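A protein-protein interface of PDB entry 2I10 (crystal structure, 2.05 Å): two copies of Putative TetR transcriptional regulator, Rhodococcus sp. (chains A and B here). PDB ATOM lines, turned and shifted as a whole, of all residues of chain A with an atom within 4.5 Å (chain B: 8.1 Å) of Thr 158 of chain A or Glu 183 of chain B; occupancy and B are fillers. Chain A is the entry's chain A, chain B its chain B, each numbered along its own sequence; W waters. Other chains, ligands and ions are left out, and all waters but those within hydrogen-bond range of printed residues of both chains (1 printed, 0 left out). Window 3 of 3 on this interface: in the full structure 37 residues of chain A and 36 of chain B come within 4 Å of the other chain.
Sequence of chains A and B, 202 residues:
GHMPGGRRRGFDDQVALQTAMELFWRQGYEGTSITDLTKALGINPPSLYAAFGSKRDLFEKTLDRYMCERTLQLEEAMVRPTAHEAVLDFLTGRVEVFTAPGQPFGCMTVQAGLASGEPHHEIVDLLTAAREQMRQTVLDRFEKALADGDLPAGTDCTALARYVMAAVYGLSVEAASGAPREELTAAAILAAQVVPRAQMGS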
ATOM      1  N   LEU A 139      10.300 -26.872  15.443  1.00  0.00           N
ATOM      2  CA  LEU A 139       9.265 -26.510  14.504  1.00  0.00           C
ATOM      3  C   LEU A 139       8.284 -27.663  14.273  1.00  0.00           C
ATOM      4  O   LEU A 139       7.061 -27.438  14.200  1.00  0.00           O
ATOM      5  CB  LEU A 139       9.918 -26.122  13.174  1.00  0.00           C
ATOM      6  CG  LEU A 139       9.069 -25.454  12.107  1.00  0.00           C
ATOM      7  CD1 LEU A 139       8.276 -24.280  12.691  1.00  0.00           C
ATOM      8  CD2 LEU A 139       9.939 -25.015  10.928  1.00  0.00           C
ATOM      9  N   ASP A 156       2.190 -18.333  15.154  1.00  0.00           N
ATOM     10  CA  ASP A 156       3.244 -18.328  14.155  1.00  0.00           C
ATOM     11  C   ASP A 156       4.358 -19.243  14.649  1.00  0.00           C
ATOM     12  O   ASP A 156       5.210 -18.836  15.454  1.00  0.00           O
ATOM     13  CB  ASP A 156       3.729 -16.894  13.923  1.00  0.00           C
ATOM     14  CG  ASP A 156       4.787 -16.789  12.841  1.00  0.00           C
ATOM     15  OD1 ASP A 156       5.484 -17.788  12.566  1.00  0.00           O
ATOM     16  OD2 ASP A 156       4.946 -15.680  12.281  1.00  0.00           O
ATOM     17  N   CYS A 157       4.333 -20.486  14.168  1.00  0.00           N
ATOM     18  CA  CYS A 157       5.237 -21.560  14.615  1.00  0.00           C
ATOM     19  C   CYS A 157       6.684 -21.328  14.185  1.00  0.00           C
ATOM     20  O   CYS A 157       7.637 -21.676  14.891  1.00  0.00           O
ATOM     21  CB  CYS A 157       4.734 -22.915  14.093  1.00  0.00           C
ATOM     22  SG  CYS A 157       3.123 -23.431  14.799  1.00  0.00           S
ATOM     23  N   THR A 158       6.842 -20.742  13.006  1.00  0.00           N
ATOM     24  CA  THR A 158       8.151 -20.340  12.513  1.00  0.00           C
ATOM     25  C   THR A 158       8.798 -19.269  13.434  1.00  0.00           C
ATOM     26  O   THR A 158       9.936 -19.442  13.859  1.00  0.00           O
ATOM     27  CB  THR A 158       8.052 -19.890  11.027  1.00  0.00           C
ATOM     28  OG1 THR A 158       7.699 -21.018  10.194  1.00  0.00           O
ATOM     29  CG2 THR A 158       9.333 -19.345  10.538  1.00  0.00           C
ATOM     30  N   ALA A 159       8.074 -18.185  13.738  1.00  0.00           N
ATOM     31  CA  ALA A 159       8.603 -17.136  14.631  1.00  0.00           C
ATOM     32  C   ALA A 159       8.789 -17.671  16.037  1.00  0.00           C
ATOM     33  O   ALA A 159       9.766 -17.317  16.695  1.00  0.00           O
ATOM     34  CB  ALA A 159       7.716 -15.918  14.665  1.00  0.00           C
ATOM     35  N   LEU A 160       7.865 -18.516  16.487  1.00  0.00           N
ATOM     36  CA  LEU A 160       7.981 -19.117  17.797  1.00  0.00           C
ATOM     37  C   LEU A 160       9.209 -20.047  17.947  1.00  0.00           C
ATOM     38  O   LEU A 160       9.857 -20.021  18.998  1.00  0.00           O
ATOM     39  CB  LEU A 160       6.681 -19.819  18.194  1.00  0.00           C
ATOM     40  CG  LEU A 160       6.521 -20.277  19.652  1.00  0.00           C
ATOM     41  CD1 LEU A 160       6.590 -19.125  20.598  1.00  0.00           C
ATOM     42  CD2 LEU A 160       5.214 -21.014  19.845  1.00  0.00           C
ATOM     43  N   ALA A 161       9.526 -20.845  16.914  1.00  0.00           N
ATOM     44  CA  ALA A 161      10.743 -21.666  16.924  1.00  0.00           C
ATOM     45  C   ALA A 161      12.033 -20.814  16.913  1.00  0.00           C
ATOM     46  O   ALA A 161      12.978 -21.114  17.647  1.00  0.00           O
ATOM     47  CB  ALA A 161      10.749 -22.677  15.783  1.00  0.00           C
ATOM     48  N   ARG A 162      12.056 -19.762  16.087  1.00  0.00           N
ATOM     49  CA  ARG A 162      13.146 -18.799  16.106  1.00  0.00           C
ATOM     50  C   ARG A 162      13.315 -18.172  17.491  1.00  0.00           C
ATOM     51  O   ARG A 162      14.413 -18.005  17.942  1.00  0.00           O
ATOM     52  CB  ARG A 162      12.930 -17.687  15.074  1.00  0.00           C
ATOM     53  CG  ARG A 162      14.122 -16.751  14.927  1.00  0.00           C
ATOM     54  CD  ARG A 162      15.322 -17.465  14.346  1.00  0.00           C
ATOM     55  NE  ARG A 162      15.039 -17.942  13.000  1.00  0.00           N
ATOM     56  CZ  ARG A 162      15.868 -18.665  12.251  1.00  0.00           C
ATOM     57  NH1 ARG A 162      17.068 -19.013  12.687  1.00  0.00           N
ATOM     58  NH2 ARG A 162      15.488 -19.044  11.049  1.00  0.00           N
ATOM     59  N   VAL B  95      17.493  -5.843  16.867  1.00  0.00           N
ATOM     60  CA  VAL B  95      17.308  -6.687  15.691  1.00  0.00           C
ATOM     61  C   VAL B  95      17.566  -5.877  14.395  1.00  0.00           C
ATOM     62  O   VAL B  95      18.113  -6.400  13.440  1.00  0.00           O
ATOM     63  CB  VAL B  95      15.904  -7.377  15.662  1.00  0.00           C
ATOM     64  CG1 VAL B  95      15.633  -8.005  14.290  1.00  0.00           C
ATOM     65  CG2 VAL B  95      15.809  -8.481  16.731  1.00  0.00           C
ATOM     66  N   LEU B 171      19.064 -13.205  20.331  1.00  0.00           N
ATOM     67  CA  LEU B 171      18.695 -12.583  19.037  1.00  0.00           C
ATOM     68  C   LEU B 171      19.931 -12.214  18.222  1.00  0.00           C
ATOM     69  O   LEU B 171      19.925 -12.376  17.012  1.00  0.00           O
ATOM     70  CB  LEU B 171      17.806 -11.362  19.225  1.00  0.00           C
ATOM     71  CG  LEU B 171      16.394 -11.644  19.729  1.00  0.00           C
ATOM     72  CD1 LEU B 171      15.856 -10.371  20.433  1.00  0.00           C
ATOM     73  CD2 LEU B 171      15.517 -12.019  18.571  1.00  0.00           C
ATOM     74  N   GLU B 174      21.183 -15.450  16.555  1.00  0.00           N
ATOM     75  CA  GLU B 174      20.338 -15.820  15.453  1.00  0.00           C
ATOM     76  C   GLU B 174      20.576 -14.942  14.240  1.00  0.00           C
ATOM     77  O   GLU B 174      20.671 -15.443  13.136  1.00  0.00           O
ATOM     78  CB  GLU B 174      18.857 -15.882  15.884  1.00  0.00           C
ATOM     79  CG  GLU B 174      18.584 -17.057  16.833  1.00  0.00           C
ATOM     80  CD  GLU B 174      18.887 -18.380  16.162  1.00  0.00           C
ATOM     81  OE1 GLU B 174      18.512 -18.588  14.990  1.00  0.00           O
ATOM     82  OE2 GLU B 174      19.559 -19.186  16.781  1.00  0.00           O
ATOM     83  N   GLY B 178      22.198 -15.796  10.296  1.00  0.00           N
ATOM     84  CA  GLY B 178      21.539 -15.547   9.024  1.00  0.00           C
ATOM     85  C   GLY B 178      20.038 -15.646   9.049  1.00  0.00           C
ATOM     86  O   GLY B 178      19.404 -15.738   7.997  1.00  0.00           O
ATOM     87  N   ALA B 179      19.452 -15.582  10.238  1.00  0.00           N
ATOM     88  CA  ALA B 179      18.006 -15.609  10.368  1.00  0.00           C
ATOM     89  C   ALA B 179      17.385 -14.437   9.596  1.00  0.00           C
ATOM     90  O   ALA B 179      17.918 -13.314   9.642  1.00  0.00           O
ATOM     91  CB  ALA B 179      17.600 -15.566  11.871  1.00  0.00           C
ATOM     92  N   PRO B 180      16.266 -14.688   8.879  1.00  0.00           N
ATOM     93  CA  PRO B 180      15.588 -13.608   8.156  1.00  0.00           C
ATOM     94  C   PRO B 180      15.153 -12.512   9.121  1.00  0.00           C
ATOM     95  O   PRO B 180      14.779 -12.804  10.275  1.00  0.00           O
ATOM     96  CB  PRO B 180      14.346 -14.290   7.549  1.00  0.00           C
ATOM     97  CG  PRO B 180      14.631 -15.718   7.550  1.00  0.00           C
ATOM     98  CD  PRO B 180      15.580 -15.981   8.697  1.00  0.00           C
ATOM     99  N   ARG B 181      15.212 -11.268   8.656  1.00  0.00           N
ATOM    100  CA  ARG B 181      14.928 -10.127   9.531  1.00  0.00           C
ATOM    101  C   ARG B 181      13.471 -10.044  10.020  1.00  0.00           C
ATOM    102  O   ARG B 181      13.247  -9.748  11.194  1.00  0.00           O
ATOM    103  CB  ARG B 181      15.467  -8.816   8.907  1.00  0.00           C
ATOM    104  CG  ARG B 181      14.500  -7.620   8.764  1.00  0.00           C
ATOM    105  CD  ARG B 181      14.687  -6.547   9.843  1.00  0.00           C
ATOM    106  NE  ARG B 181      16.020  -5.925   9.820  1.00  0.00           N
ATOM    107  CZ  ARG B 181      16.299  -4.679   9.430  1.00  0.00           C
ATOM    108  NH1 ARG B 181      15.334  -3.858   9.004  1.00  0.00           N
ATOM    109  NH2 ARG B 181      17.557  -4.246   9.479  1.00  0.00           N
ATOM    110  N   GLU B 182      12.480 -10.311   9.165  1.00  0.00           N
ATOM    111  CA  GLU B 182      11.072 -10.259   9.581  1.00  0.00           C
ATOM    112  C   GLU B 182      10.775 -11.335  10.638  1.00  0.00           C
ATOM    113  O   GLU B 182      10.019 -11.115  11.611  1.00  0.00           O
ATOM    114  CB  GLU B 182      10.128 -10.375   8.369  1.00  0.00           C
ATOM    115  CG  GLU B 182      10.331  -9.272   7.302  1.00  0.00           C
ATOM    116  CD  GLU B 182       9.336  -9.323   6.138  1.00  0.00           C
ATOM    117  OE1 GLU B 182       8.223  -9.883   6.294  1.00  0.00           O
ATOM    118  OE2 GLU B 182       9.672  -8.787   5.055  1.00  0.00           O
ATOM    119  N   GLU B 183      11.375 -12.499  10.444  1.00  0.00           N
ATOM    120  CA  GLU B 183      11.263 -13.577  11.407  1.00  0.00           C
ATOM    121  C   GLU B 183      11.926 -13.218  12.755  1.00  0.00           C
ATOM    122  O   GLU B 183      11.384 -13.527  13.833  1.00  0.00           O
ATOM    123  CB  GLU B 183      11.910 -14.812  10.820  1.00  0.00           C
ATOM    124  CG  GLU B 183      11.775 -16.047  11.642  1.00  0.00           C
ATOM    125  CD  GLU B 183      12.169 -17.279  10.860  1.00  0.00           C
ATOM    126  OE1 GLU B 183      11.727 -17.414   9.711  1.00  0.00           O
ATOM    127  OE2 GLU B 183      12.904 -18.117  11.407  1.00  0.00           O
ATOM    128  N   LEU B 184      13.103 -12.601  12.709  1.00  0.00           N
ATOM    129  CA  LEU B 184      13.803 -12.232  13.944  1.00  0.00           C
ATOM    130  C   LEU B 184      13.066 -11.122  14.702  1.00  0.00           C
ATOM    131  O   LEU B 184      13.013 -11.120  15.940  1.00  0.00           O
ATOM    132  CB  LEU B 184      15.274 -11.848  13.673  1.00  0.00           C
ATOM    133  CG  LEU B 184      16.229 -12.168  14.820  1.00  0.00           C
ATOM    134  CD1 LEU B 184      16.099 -13.624  15.283  1.00  0.00           C
ATOM    135  CD2 LEU B 184      17.677 -11.839  14.476  1.00  0.00           C
ATOM    136  N   THR B 185      12.488 -10.189  13.951  1.00  0.00           N
ATOM    137  CA  THR B 185      11.677  -9.128  14.521  1.00  0.00           C
ATOM    138  C   THR B 185      10.442  -9.720  15.208  1.00  0.00           C
ATOM    139  O   THR B 185      10.108  -9.297  16.323  1.00  0.00           O
ATOM    140  CB  THR B 185      11.275  -8.108  13.419  1.00  0.00           C
ATOM    141  OG1 THR B 185      12.453  -7.403  12.998  1.00  0.00           O
ATOM    142  CG2 THR B 185      10.227  -7.119  13.934  1.00  0.00           C
ATOM    143  N   ALA B 186       9.780 -10.694  14.554  1.00  0.00           N
ATOM    144  CA  ALA B 186       8.665 -11.406  15.182  1.00  0.00           C
ATOM    145  C   ALA B 186       9.134 -12.107  16.467  1.00  0.00           C
ATOM    146  O   ALA B 186       8.479 -12.010  17.494  1.00  0.00           O
ATOM    147  CB  ALA B 186       7.980 -12.388  14.201  1.00  0.00           C
ATOM    148  N   ALA B 187      10.299 -12.737  16.440  1.00  0.00           N
ATOM    149  CA  ALA B 187      10.865 -13.346  17.633  1.00  0.00           C
ATOM    150  C   ALA B 187      11.121 -12.349  18.782  1.00  0.00           C
ATOM    151  O   ALA B 187      10.886 -12.694  19.956  1.00  0.00           O
ATOM    152  CB  ALA B 187      12.148 -14.103  17.299  1.00  0.00           C
ATOM    153  N   ALA B 188      11.625 -11.153  18.452  1.00  0.00           N
ATOM    154  CA  ALA B 188      11.899 -10.124  19.475  1.00  0.00           C
ATOM    155  C   ALA B 188      10.600  -9.618  20.116  1.00  0.00           C
ATOM    156  O   ALA B 188      10.559  -9.396  21.310  1.00  0.00           O
ATOM    157  CB  ALA B 188      12.680  -8.986  18.867  1.00  0.00           C
ATOM    158  N   ILE B 189       9.543  -9.465  19.304  1.00  0.00           N
ATOM    159  CA  ILE B 189       8.206  -9.126  19.768  1.00  0.00           C
ATOM    160  C   ILE B 189       7.656 -10.192  20.723  1.00  0.00           C
ATOM    161  O   ILE B 189       7.119  -9.852  21.774  1.00  0.00           O
ATOM    162  CB  ILE B 189       7.228  -8.869  18.595  1.00  0.00           C
ATOM    163  CG1 ILE B 189       7.603  -7.552  17.899  1.00  0.00           C
ATOM    164  CG2 ILE B 189       5.780  -8.798  19.078  1.00  0.00           C
ATOM    165  CD1 ILE B 189       6.893  -7.301  16.525  1.00  0.00           C
ATOM    166  N   LEU B 190       7.800 -11.472  20.378  1.00  0.00           N
ATOM    167  CA  LEU B 190       7.448 -12.550  21.328  1.00  0.00           C
ATOM    168  C   LEU B 190       8.303 -12.501  22.597  1.00  0.00           C
ATOM    169  O   LEU B 190       7.805 -12.720  23.711  1.00  0.00           O
ATOM    170  CB  LEU B 190       7.610 -13.910  20.657  1.00  0.00           C
ATOM    171  CG  LEU B 190       6.686 -14.268  19.500  1.00  0.00           C
ATOM    172  CD1 LEU B 190       7.199 -15.526  18.820  1.00  0.00           C
ATOM    173  CD2 LEU B 190       5.281 -14.476  20.019  1.00  0.00           C
HETATM  174  O   HOH W   1      12.276 -20.525  12.543  1.00  0.00           O
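OE1 of Glu 174 of chain B is in salt-bridge range of NH1 of Arg 162 of chain A, 2.8 Å away.
The side-chain carboxylate (OE2) of Glu 183 of chain B lies within salt-bridge range of the guanidinium group (NE) of Arg 162 of chain A, 2.7 Å away.
The side-chain carboxylate (OD1) of Asp 156 of chain A sits at hydrogen-bond distance from the backbone NH (N) of Thr 158 of chain A (3.3 Å).
The backbone NH of Ala 159 of chain A is in hydrogen-bond range of the side-chain carboxylate of Asp 156 of chain A (2.9 Å).
The backbone carbonyl oxygen (O) of Glu 174 of chain B is in hydrogen-bond range of the backbone NH (N) of Ala 179 of chain B, at 3.1 Å.
Among the printed residues, pairs that only touch across the chains: Thr 158 of chain A with Glu 183 of chain B (3.2 Å), Ala 159 of chain A with Ala 186 of chain B (3.6 Å), Ala 159 of chain A with Leu 190 of chain B (3.8 Å), Leu 160 of chain A with Leu 190 of chain B (3.8 Å), Arg 162 of chain A with Ala 179 of chain B (3.6 Å), Arg 162 of chain A with Pro 180 of chain B (3.9 Å) and Arg 162 of chain A with Leu 184 of chain B (3.7 Å).
Of chain B, only Glu 183 comes within 4 Å of Thr 158 of chain A.
Val 95 of chain B touches none of the printed residues of chain A.
Printed residues of chain A within 4 Å of Glu 174 of chain B: Arg 162 (2.8 Å).
Of chain A, only Thr 158 (3.2 Å) and Arg 162 (2.7 Å) come within 4 Å of Glu 183 of chain B.
Ala 188 of chain B touches none of the printed residues of chain A.
Printed residues of chain A within 4 Å of Leu 190 of chain B: Ala 159 and Leu 160.
The nearest printed residue of chain B that does not touch Thr 158 of chain A is Ala 187 of chain B (6.7 Å).
Along chain A the printed residues that touch a printed residue of chain B span positions 158 to 162.
Of the 16 printed residues of chain B, 7 touch a printed residue of chain A.
Hydrophobic or aromatic side chains of chain B within 4 Å of the printed part of chain A: Ala 179, Pro 180, Leu 184, Ala 186 and Leu 190.
No position is printed for both chains.
Water W1 lies within hydrogen-bond range of OE2 of Glu 183 of chain B and O of Thr 158 of chain A.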
